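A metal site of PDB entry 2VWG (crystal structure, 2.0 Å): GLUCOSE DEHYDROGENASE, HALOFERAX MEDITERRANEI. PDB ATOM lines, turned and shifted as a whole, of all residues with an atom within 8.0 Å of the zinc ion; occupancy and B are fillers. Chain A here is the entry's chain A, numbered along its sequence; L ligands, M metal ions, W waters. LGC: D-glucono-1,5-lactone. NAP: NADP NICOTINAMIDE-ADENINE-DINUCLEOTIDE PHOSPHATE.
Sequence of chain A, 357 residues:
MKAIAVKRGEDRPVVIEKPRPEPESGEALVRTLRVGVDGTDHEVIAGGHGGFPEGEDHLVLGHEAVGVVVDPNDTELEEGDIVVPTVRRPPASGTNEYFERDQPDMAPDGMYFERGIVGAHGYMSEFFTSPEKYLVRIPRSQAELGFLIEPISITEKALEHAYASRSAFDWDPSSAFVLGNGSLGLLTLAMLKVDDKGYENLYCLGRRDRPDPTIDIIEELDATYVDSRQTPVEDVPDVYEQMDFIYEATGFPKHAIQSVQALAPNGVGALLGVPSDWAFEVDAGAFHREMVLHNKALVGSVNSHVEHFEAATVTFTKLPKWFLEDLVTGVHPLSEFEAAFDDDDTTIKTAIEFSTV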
ATOM      1  N   GLY A  36      22.134  -6.979   1.579  1.00  0.00           N
ATOM      2  CA  GLY A  36      21.340  -8.113   1.131  1.00  0.00           C
ATOM      3  C   GLY A  36      20.157  -7.688   0.278  1.00  0.00           C
ATOM      4  O   GLY A  36      19.738  -6.526   0.288  1.00  0.00           O
ATOM      5  N   VAL A  37      19.622  -8.653  -0.460  1.00  0.00           N
ATOM      6  CA  VAL A  37      18.418  -8.457  -1.278  1.00  0.00           C
ATOM      7  C   VAL A  37      17.386  -9.466  -0.830  1.00  0.00           C
ATOM      8  O   VAL A  37      17.732 -10.601  -0.495  1.00  0.00           O
ATOM      9  CB  VAL A  37      18.732  -8.690  -2.785  1.00  0.00           C
ATOM     10  CG1 VAL A  37      17.456  -8.549  -3.620  1.00  0.00           C
ATOM     11  CG2 VAL A  37      19.786  -7.733  -3.251  1.00  0.00           C
ATOM     12  N   ASP A  38      16.119  -9.070  -0.782  1.00  0.00           N
ATOM     13  CA  ASP A  38      15.053 -10.030  -0.427  1.00  0.00           C
ATOM     14  C   ASP A  38      13.792  -9.808  -1.260  1.00  0.00           C
ATOM     15  O   ASP A  38      13.769  -8.955  -2.150  1.00  0.00           O
ATOM     16  CB  ASP A  38      14.760 -10.027   1.088  1.00  0.00           C
ATOM     17  CG  ASP A  38      13.968  -8.807   1.550  1.00  0.00           C
ATOM     18  OD1 ASP A  38      13.741  -7.892   0.748  1.00  0.00           O
ATOM     19  OD2 ASP A  38      13.589  -8.756   2.728  1.00  0.00           O
ATOM     20  N   GLY A  39      12.769 -10.601  -0.958  1.00  0.00           N
ATOM     21  CA  GLY A  39      11.482 -10.511  -1.622  1.00  0.00           C
ATOM     22  C   GLY A  39      10.868  -9.131  -1.575  1.00  0.00           C
ATOM     23  O   GLY A  39      10.241  -8.704  -2.527  1.00  0.00           O
ATOM     24  N   THR A  40      11.022  -8.429  -0.454  1.00  0.00           N
ATOM     25  CA  THR A  40      10.483  -7.074  -0.309  1.00  0.00           C
ATOM     26  C   THR A  40      11.112  -6.130  -1.338  1.00  0.00           C
ATOM     27  O   THR A  40      10.412  -5.302  -1.926  1.00  0.00           O
ATOM     28  CB  THR A  40      10.703  -6.527   1.105  1.00  0.00           C
ATOM     29  OG1 THR A  40      10.106  -7.427   2.070  1.00  0.00           O
ATOM     30  CG2 THR A  40      10.092  -5.127   1.230  1.00  0.00           C
ATOM     31  N   ASP A  41      12.423  -6.242  -1.553  1.00  0.00           N
ATOM     32  CA  ASP A  41      13.108  -5.392  -2.545  1.00  0.00           C
ATOM     33  C   ASP A  41      12.548  -5.582  -3.968  1.00  0.00           C
ATOM     34  O   ASP A  41      12.441  -4.627  -4.734  1.00  0.00           O
ATOM     35  CB  ASP A  41      14.611  -5.676  -2.584  1.00  0.00           C
ATOM     36  CG  ASP A  41      15.307  -5.322  -1.273  1.00  0.00           C
ATOM     37  OD1 ASP A  41      15.013  -4.262  -0.716  1.00  0.00           O
ATOM     38  OD2 ASP A  41      16.110  -6.140  -0.801  1.00  0.00           O
ATOM     39  N   GLY A  62      17.778  -1.165  -0.732  1.00  0.00           N
ATOM     40  CA  GLY A  62      18.562  -1.883   0.255  1.00  0.00           C
ATOM     41  C   GLY A  62      18.184  -1.511   1.676  1.00  0.00           C
ATOM     42  O   GLY A  62      18.292  -0.361   2.077  1.00  0.00           O
ATOM     43  N   HIS A  63      17.743  -2.508   2.445  1.00  0.00           N
ATOM     44  CA  HIS A  63      17.408  -2.288   3.847  1.00  0.00           C
ATOM     45  C   HIS A  63      18.117  -3.256   4.788  1.00  0.00           C
ATOM     46  O   HIS A  63      17.975  -3.151   5.996  1.00  0.00           O
ATOM     47  CB  HIS A  63      15.885  -2.331   4.019  1.00  0.00           C
ATOM     48  CG  HIS A  63      15.284  -3.656   3.677  1.00  0.00           C
ATOM     49  ND1 HIS A  63      14.883  -3.974   2.396  1.00  0.00           N
ATOM     50  CD2 HIS A  63      15.078  -4.766   4.429  1.00  0.00           C
ATOM     51  CE1 HIS A  63      14.432  -5.223   2.390  1.00  0.00           C
ATOM     52  NE2 HIS A  63      14.531  -5.712   3.599  1.00  0.00           N
ATOM     53  N   GLU A  64      18.889  -4.196   4.226  1.00  0.00           N
ATOM     54  CA  GLU A  64      19.615  -5.209   4.956  1.00  0.00           C
ATOM     55  C   GLU A  64      21.115  -4.938   4.755  1.00  0.00           C
ATOM     56  O   GLU A  64      21.702  -5.419   3.791  1.00  0.00           O
ATOM     57  CB  GLU A  64      19.321  -6.605   4.411  1.00  0.00           C
ATOM     58  CG  GLU A  64      17.844  -7.034   4.380  1.00  0.00           C
ATOM     59  CD  GLU A  64      17.669  -8.411   3.778  1.00  0.00           C
ATOM     60  OE1 GLU A  64      18.647  -8.980   3.221  1.00  0.00           O
ATOM     61  OE2 GLU A  64      16.545  -8.953   3.857  1.00  0.00           O
ATOM     62  N   ALA A  65      21.726  -4.202   5.657  1.00  0.00           N
ATOM     63  CA  ALA A  65      23.080  -3.690   5.420  1.00  0.00           C
ATOM     64  C   ALA A  65      24.006  -3.948   6.585  1.00  0.00           C
ATOM     65  O   ALA A  65      23.587  -4.044   7.727  1.00  0.00           O
ATOM     66  CB  ALA A  65      23.013  -2.201   5.165  1.00  0.00           C
ATOM     67  N   VAL A  87      15.951   0.040  10.228  1.00  0.00           N
ATOM     68  CA  VAL A  87      15.320   0.433   8.996  1.00  0.00           C
ATOM     69  C   VAL A  87      14.413   1.671   9.133  1.00  0.00           C
ATOM     70  O   VAL A  87      14.366   2.500   8.226  1.00  0.00           O
ATOM     71  CB  VAL A  87      14.567  -0.747   8.394  1.00  0.00           C
ATOM     72  CG1 VAL A  87      13.758  -0.332   7.143  1.00  0.00           C
ATOM     73  CG2 VAL A  87      15.579  -1.871   8.064  1.00  0.00           C
ATOM     74  N   ILE A 117      12.746   1.393   1.322  1.00  0.00           N
ATOM     75  CA  ILE A 117      11.432   0.820   1.109  1.00  0.00           C
ATOM     76  C   ILE A 117      10.375   1.923   0.930  1.00  0.00           C
ATOM     77  O   ILE A 117       9.701   1.977  -0.093  1.00  0.00           O
ATOM     78  CB  ILE A 117      11.015  -0.111   2.261  1.00  0.00           C
ATOM     79  CG1 ILE A 117      12.073  -1.188   2.495  1.00  0.00           C
ATOM     80  CG2 ILE A 117       9.664  -0.790   1.943  1.00  0.00           C
ATOM     81  CD1 ILE A 117      11.756  -2.124   3.656  1.00  0.00           C
ATOM     82  N   PHE A 147      24.645  -8.737   6.846  1.00  0.00           N
ATOM     83  CA  PHE A 147      23.376  -8.351   6.212  1.00  0.00           C
ATOM     84  C   PHE A 147      22.257  -9.313   6.577  1.00  0.00           C
ATOM     85  O   PHE A 147      21.107  -9.043   6.279  1.00  0.00           O
ATOM     86  CB  PHE A 147      23.510  -8.254   4.667  1.00  0.00           C
ATOM     87  CG  PHE A 147      23.956  -9.532   4.006  1.00  0.00           C
ATOM     88  CD1 PHE A 147      23.043 -10.491   3.622  1.00  0.00           C
ATOM     89  CD2 PHE A 147      25.307  -9.783   3.785  1.00  0.00           C
ATOM     90  CE1 PHE A 147      23.456 -11.669   3.053  1.00  0.00           C
ATOM     91  CE2 PHE A 147      25.723 -10.952   3.200  1.00  0.00           C
ATOM     92  CZ  PHE A 147      24.798 -11.910   2.836  1.00  0.00           C
ATOM     93  N   GLU A 150      19.531  -8.227   9.947  1.00  0.00           N
ATOM     94  CA  GLU A 150      18.220  -7.601   9.824  1.00  0.00           C
ATOM     95  C   GLU A 150      17.083  -8.628   9.632  1.00  0.00           C
ATOM     96  O   GLU A 150      16.101  -8.593  10.377  1.00  0.00           O
ATOM     97  CB  GLU A 150      18.218  -6.497   8.751  1.00  0.00           C
ATOM     98  CG  GLU A 150      16.983  -5.610   8.769  1.00  0.00           C
ATOM     99  CD  GLU A 150      15.816  -6.155   7.973  1.00  0.00           C
ATOM    100  OE1 GLU A 150      15.992  -7.116   7.191  1.00  0.00           O
ATOM    101  OE2 GLU A 150      14.692  -5.610   8.124  1.00  0.00           O
ATOM    102  N   PRO A 151      17.197  -9.526   8.640  1.00  0.00           N
ATOM    103  CA  PRO A 151      16.128 -10.534   8.498  1.00  0.00           C
ATOM    104  C   PRO A 151      15.969 -11.469   9.699  1.00  0.00           C
ATOM    105  O   PRO A 151      14.850 -11.851  10.016  1.00  0.00           O
ATOM    106  CB  PRO A 151      16.515 -11.292   7.223  1.00  0.00           C
ATOM    107  CG  PRO A 151      17.901 -10.859   6.892  1.00  0.00           C
ATOM    108  CD  PRO A 151      18.188  -9.582   7.543  1.00  0.00           C
ATOM    109  N   ILE A 152      17.070 -11.818  10.366  1.00  0.00           N
ATOM    110  CA  ILE A 152      16.987 -12.574  11.600  1.00  0.00           C
ATOM    111  C   ILE A 152      16.178 -11.793  12.630  1.00  0.00           C
ATOM    112  O   ILE A 152      15.328 -12.353  13.315  1.00  0.00           O
ATOM    113  CB  ILE A 152      18.374 -12.932  12.177  1.00  0.00           C
ATOM    114  CG1 ILE A 152      19.104 -13.908  11.239  1.00  0.00           C
ATOM    115  CG2 ILE A 152      18.220 -13.624  13.557  1.00  0.00           C
ATOM    116  CD1 ILE A 152      20.532 -14.221  11.674  1.00  0.00           C
ATOM    117  N   ILE A 154      13.802  -9.713  12.222  1.00  0.00           N
ATOM    118  CA  ILE A 154      12.384  -9.785  11.860  1.00  0.00           C
ATOM    119  C   ILE A 154      11.707 -10.960  12.569  1.00  0.00           C
ATOM    120  O   ILE A 154      10.649 -10.810  13.191  1.00  0.00           O
ATOM    121  CB  ILE A 154      12.202  -9.914  10.301  1.00  0.00           C
ATOM    122  CG1 ILE A 154      12.656  -8.628   9.590  1.00  0.00           C
ATOM    123  CG2 ILE A 154      10.733 -10.275   9.893  1.00  0.00           C
ATOM    124  CD1 ILE A 154      11.968  -7.372  10.063  1.00  0.00           C
ATOM    125  N   SER A 183      14.117 -16.864   1.447  1.00  0.00           N
ATOM    126  CA  SER A 183      15.223 -16.660   2.368  1.00  0.00           C
ATOM    127  C   SER A 183      14.714 -16.413   3.796  1.00  0.00           C
ATOM    128  O   SER A 183      15.321 -16.900   4.757  1.00  0.00           O
ATOM    129  CB  SER A 183      16.118 -15.507   1.905  1.00  0.00           C
ATOM    130  OG  SER A 183      15.361 -14.327   1.761  1.00  0.00           O
ATOM    131  N   LEU A 184      13.600 -15.696   3.952  1.00  0.00           N
ATOM    132  CA  LEU A 184      13.052 -15.491   5.303  1.00  0.00           C
ATOM    133  C   LEU A 184      12.540 -16.800   5.923  1.00  0.00           C
ATOM    134  O   LEU A 184      12.792 -17.085   7.099  1.00  0.00           O
ATOM    135  CB  LEU A 184      11.924 -14.429   5.310  1.00  0.00           C
ATOM    136  CG  LEU A 184      11.399 -14.036   6.704  1.00  0.00           C
ATOM    137  CD1 LEU A 184      12.501 -13.444   7.582  1.00  0.00           C
ATOM    138  CD2 LEU A 184      10.217 -13.072   6.579  1.00  0.00           C
ATOM    139  N   LYS A 349      19.530 -16.529  -1.164  1.00  0.00           N
ATOM    140  CA  LYS A 349      19.857 -15.212  -0.618  1.00  0.00           C
ATOM    141  C   LYS A 349      21.052 -14.644  -1.361  1.00  0.00           C
ATOM    142  O   LYS A 349      22.089 -15.299  -1.475  1.00  0.00           O
ATOM    143  CB  LYS A 349      20.184 -15.277   0.863  1.00  0.00           C
ATOM    144  CG  LYS A 349      20.354 -13.942   1.533  1.00  0.00           C
ATOM    145  CD  LYS A 349      19.014 -13.266   1.675  1.00  0.00           C
ATOM    146  CE  LYS A 349      19.126 -11.922   2.274  1.00  0.00           C
ATOM    147  NZ  LYS A 349      17.793 -11.262   2.280  1.00  0.00           N
HETATM  148  C1  LGC L   1      10.961  -5.756   5.193  1.00  0.00           C
HETATM  149  C2  LGC L   1      11.857  -5.222   6.251  1.00  0.00           C
HETATM  150  O5  LGC L   1       9.632  -5.297   5.033  1.00  0.00           O
HETATM  151  O1  LGC L   1      11.390  -6.596   4.408  1.00  0.00           O
HETATM  152  O2  LGC L   1      12.653  -6.268   6.761  1.00  0.00           O
HETATM  153  C3  LGC L   1      11.119  -4.545   7.394  1.00  0.00           C
HETATM  154  O3  LGC L   1      12.026  -3.701   8.087  1.00  0.00           O
HETATM  155  C4  LGC L   1       9.960  -3.706   6.888  1.00  0.00           C
HETATM  156  O4  LGC L   1       9.313  -3.158   8.013  1.00  0.00           O
HETATM  157  C5  LGC L   1       8.997  -4.595   6.093  1.00  0.00           C
HETATM  158  C6  LGC L   1       7.831  -3.783   5.523  1.00  0.00           C
HETATM  159  O6  LGC L   1       8.320  -2.832   4.608  1.00  0.00           O
HETATM  160  PA  NAP L   2      10.535 -14.645  -1.212  1.00  0.00           P
HETATM  161  O1A NAP L   2      11.987 -14.869  -1.407  1.00  0.00           O
HETATM  162  O2A NAP L   2       9.721 -14.164  -2.326  1.00  0.00           O
HETATM  163  O5B NAP L   2       9.951 -16.024  -0.643  1.00  0.00           O
HETATM  164  C5B NAP L   2       8.590 -16.306  -0.760  1.00  0.00           C
HETATM  165  C4B NAP L   2       8.469 -17.790  -0.997  1.00  0.00           C
HETATM  166  O4B NAP L   2       7.145 -18.204  -0.793  1.00  0.00           O
HETATM  167  C3B NAP L   2       8.892 -18.170  -2.421  1.00  0.00           C
HETATM  168  O3B NAP L   2       9.987 -19.058  -2.396  1.00  0.00           O
HETATM  169  C2B NAP L   2       7.639 -18.822  -2.976  1.00  0.00           C
HETATM  170  O2B NAP L   2       7.918 -19.939  -3.756  1.00  0.00           O
HETATM  171  C1B NAP L   2       6.854 -19.212  -1.721  1.00  0.00           C
HETATM  172  N9A NAP L   2       5.417 -19.307  -2.019  1.00  0.00           N
HETATM  173  C8A NAP L   2       4.584 -18.317  -2.472  1.00  0.00           C
HETATM  174  N7A NAP L   2       3.345 -18.838  -2.610  1.00  0.00           N
HETATM  175  C5A NAP L   2       3.386 -20.136  -2.257  1.00  0.00           C
HETATM  176  C6A NAP L   2       2.410 -21.130  -2.221  1.00  0.00           C
HETATM  177  N6A NAP L   2       1.172 -20.871  -2.581  1.00  0.00           N
HETATM  178  N1A NAP L   2       2.769 -22.386  -1.805  1.00  0.00           N
HETATM  179  C2A NAP L   2       4.066 -22.668  -1.409  1.00  0.00           C
HETATM  180  N3A NAP L   2       5.023 -21.676  -1.456  1.00  0.00           N
HETATM  181  C4A NAP L   2       4.679 -20.439  -1.867  1.00  0.00           C
HETATM  182  O3  NAP L   2      10.337 -13.624   0.010  1.00  0.00           O
HETATM  183  PN  NAP L   2      11.150 -13.509   1.386  1.00  0.00           P
HETATM  184  O1N NAP L   2      11.495 -14.852   1.933  1.00  0.00           O
HETATM  185  O2N NAP L   2      12.215 -12.491   1.265  1.00  0.00           O
HETATM  186  O5D NAP L   2       9.937 -12.904   2.261  1.00  0.00           O
HETATM  187  C5D NAP L   2       8.744 -13.644   2.390  1.00  0.00           C
HETATM  188  C4D NAP L   2       7.572 -12.706   2.647  1.00  0.00           C
HETATM  189  O4D NAP L   2       7.771 -12.020   3.874  1.00  0.00           O
HETATM  190  C3D NAP L   2       7.404 -11.628   1.579  1.00  0.00           C
HETATM  191  O3D NAP L   2       6.015 -11.382   1.428  1.00  0.00           O
HETATM  192  C2D NAP L   2       8.080 -10.430   2.191  1.00  0.00           C
HETATM  193  O2D NAP L   2       7.608  -9.230   1.677  1.00  0.00           O
HETATM  194  C1D NAP L   2       7.693 -10.627   3.664  1.00  0.00           C
HETATM  195  N1N NAP L   2       8.561  -9.953   4.636  1.00  0.00           N
HETATM  196  C2N NAP L   2       7.952  -9.276   5.646  1.00  0.00           C
HETATM  197  C3N NAP L   2       8.692  -8.667   6.627  1.00  0.00           C
HETATM  198  C7N NAP L   2       7.987  -8.123   7.828  1.00  0.00           C
HETATM  199  O7N NAP L   2       8.622  -7.127   8.533  1.00  0.00           O
HETATM  200  N7N NAP L   2       6.766  -8.571   8.137  1.00  0.00           N
HETATM  201  C4N NAP L   2      10.074  -8.706   6.572  1.00  0.00           C
HETATM  202  C5N NAP L   2      10.691  -9.416   5.537  1.00  0.00           C
HETATM  203  C6N NAP L   2       9.921 -10.045   4.567  1.00  0.00           C
HETATM  204  P2B NAP L   2       8.171 -19.833  -5.356  1.00  0.00           P
HETATM  205  O1X NAP L   2       9.519 -19.245  -5.552  1.00  0.00           O
HETATM  206  O2X NAP L   2       7.125 -19.008  -6.019  1.00  0.00           O
HETATM  207  O3X NAP L   2       8.157 -21.286  -5.799  1.00  0.00           O
HETATM  208 ZN    ZN M   1      14.779  -7.774   4.144  1.00  0.00          ZN
HETATM  209  O   HOH W   1      14.285  -8.108   5.862  1.00  0.00           O
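Glu 150 touches the zinc ion (OE1 to ZN, 3.3 Å). Within 4 Å of the zinc ion: Asp 38, His 63, Glu 64 and Glu 150.
An oxygen (O1) of LGC L1 sits close to a ring nitrogen (NE2) of His 63, at 3.4 Å. The side-chain carboxylate of Glu 150 lies within hydrogen-bond range of an oxygen (O2) of LGC L1, at 2.5 Å. An oxygen (O1) of LGC L1 is in hydrogen-bond range of the side-chain hydroxyl (OG1) of Thr 40, at 2.8 Å. OG1 of Thr 40 lies within hydrogen-bond range of O2D of NAP L2, 3.1 Å away. The backbone NH of Gly 39 sits at hydrogen-bond distance from an oxygen (O2N) of NAP L2. The backbone NH of Ser 183 lies within hydrogen-bond range of an oxygen (O1N) of NAP L2 (3.3 Å). N of Leu 184 lies within hydrogen-bond range of O1N of NAP L2, 3.0 Å away.
Water W1 bridges an oxygen (O2) of LGC L1 (2.6 Å) and the side-chain carboxylate (OE2) of Glu 150 (3.4 Å).
The zinc ion is bound by water W1 (1.8 Å), OD2 of Asp 38 (2.1 Å), OE2 of Glu 64 (2.1 Å) and NE2 of His 63 (2.1 Å). The zinc ion has four donor atoms within binding distance.
OD1 of Asp 38 lies within hydrogen-bond range of N of Thr 40. The backbone NH of Asp 38 sits at hydrogen-bond distance from the side-chain carboxylate of Asp 41, at 2.9 Å. The side-chain carboxylate of Glu 64 is in salt-bridge range of the side-chain amino group of Lys 349 (2.6 Å). O of Glu 64 sits at hydrogen-bond distance from N of Gly 36, at 2.7 Å. A ring nitrogen (ND1) of His 63 lies within hydrogen-bond range of the side-chain carboxylate (OD1) of Asp 41 (3.1 Å).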
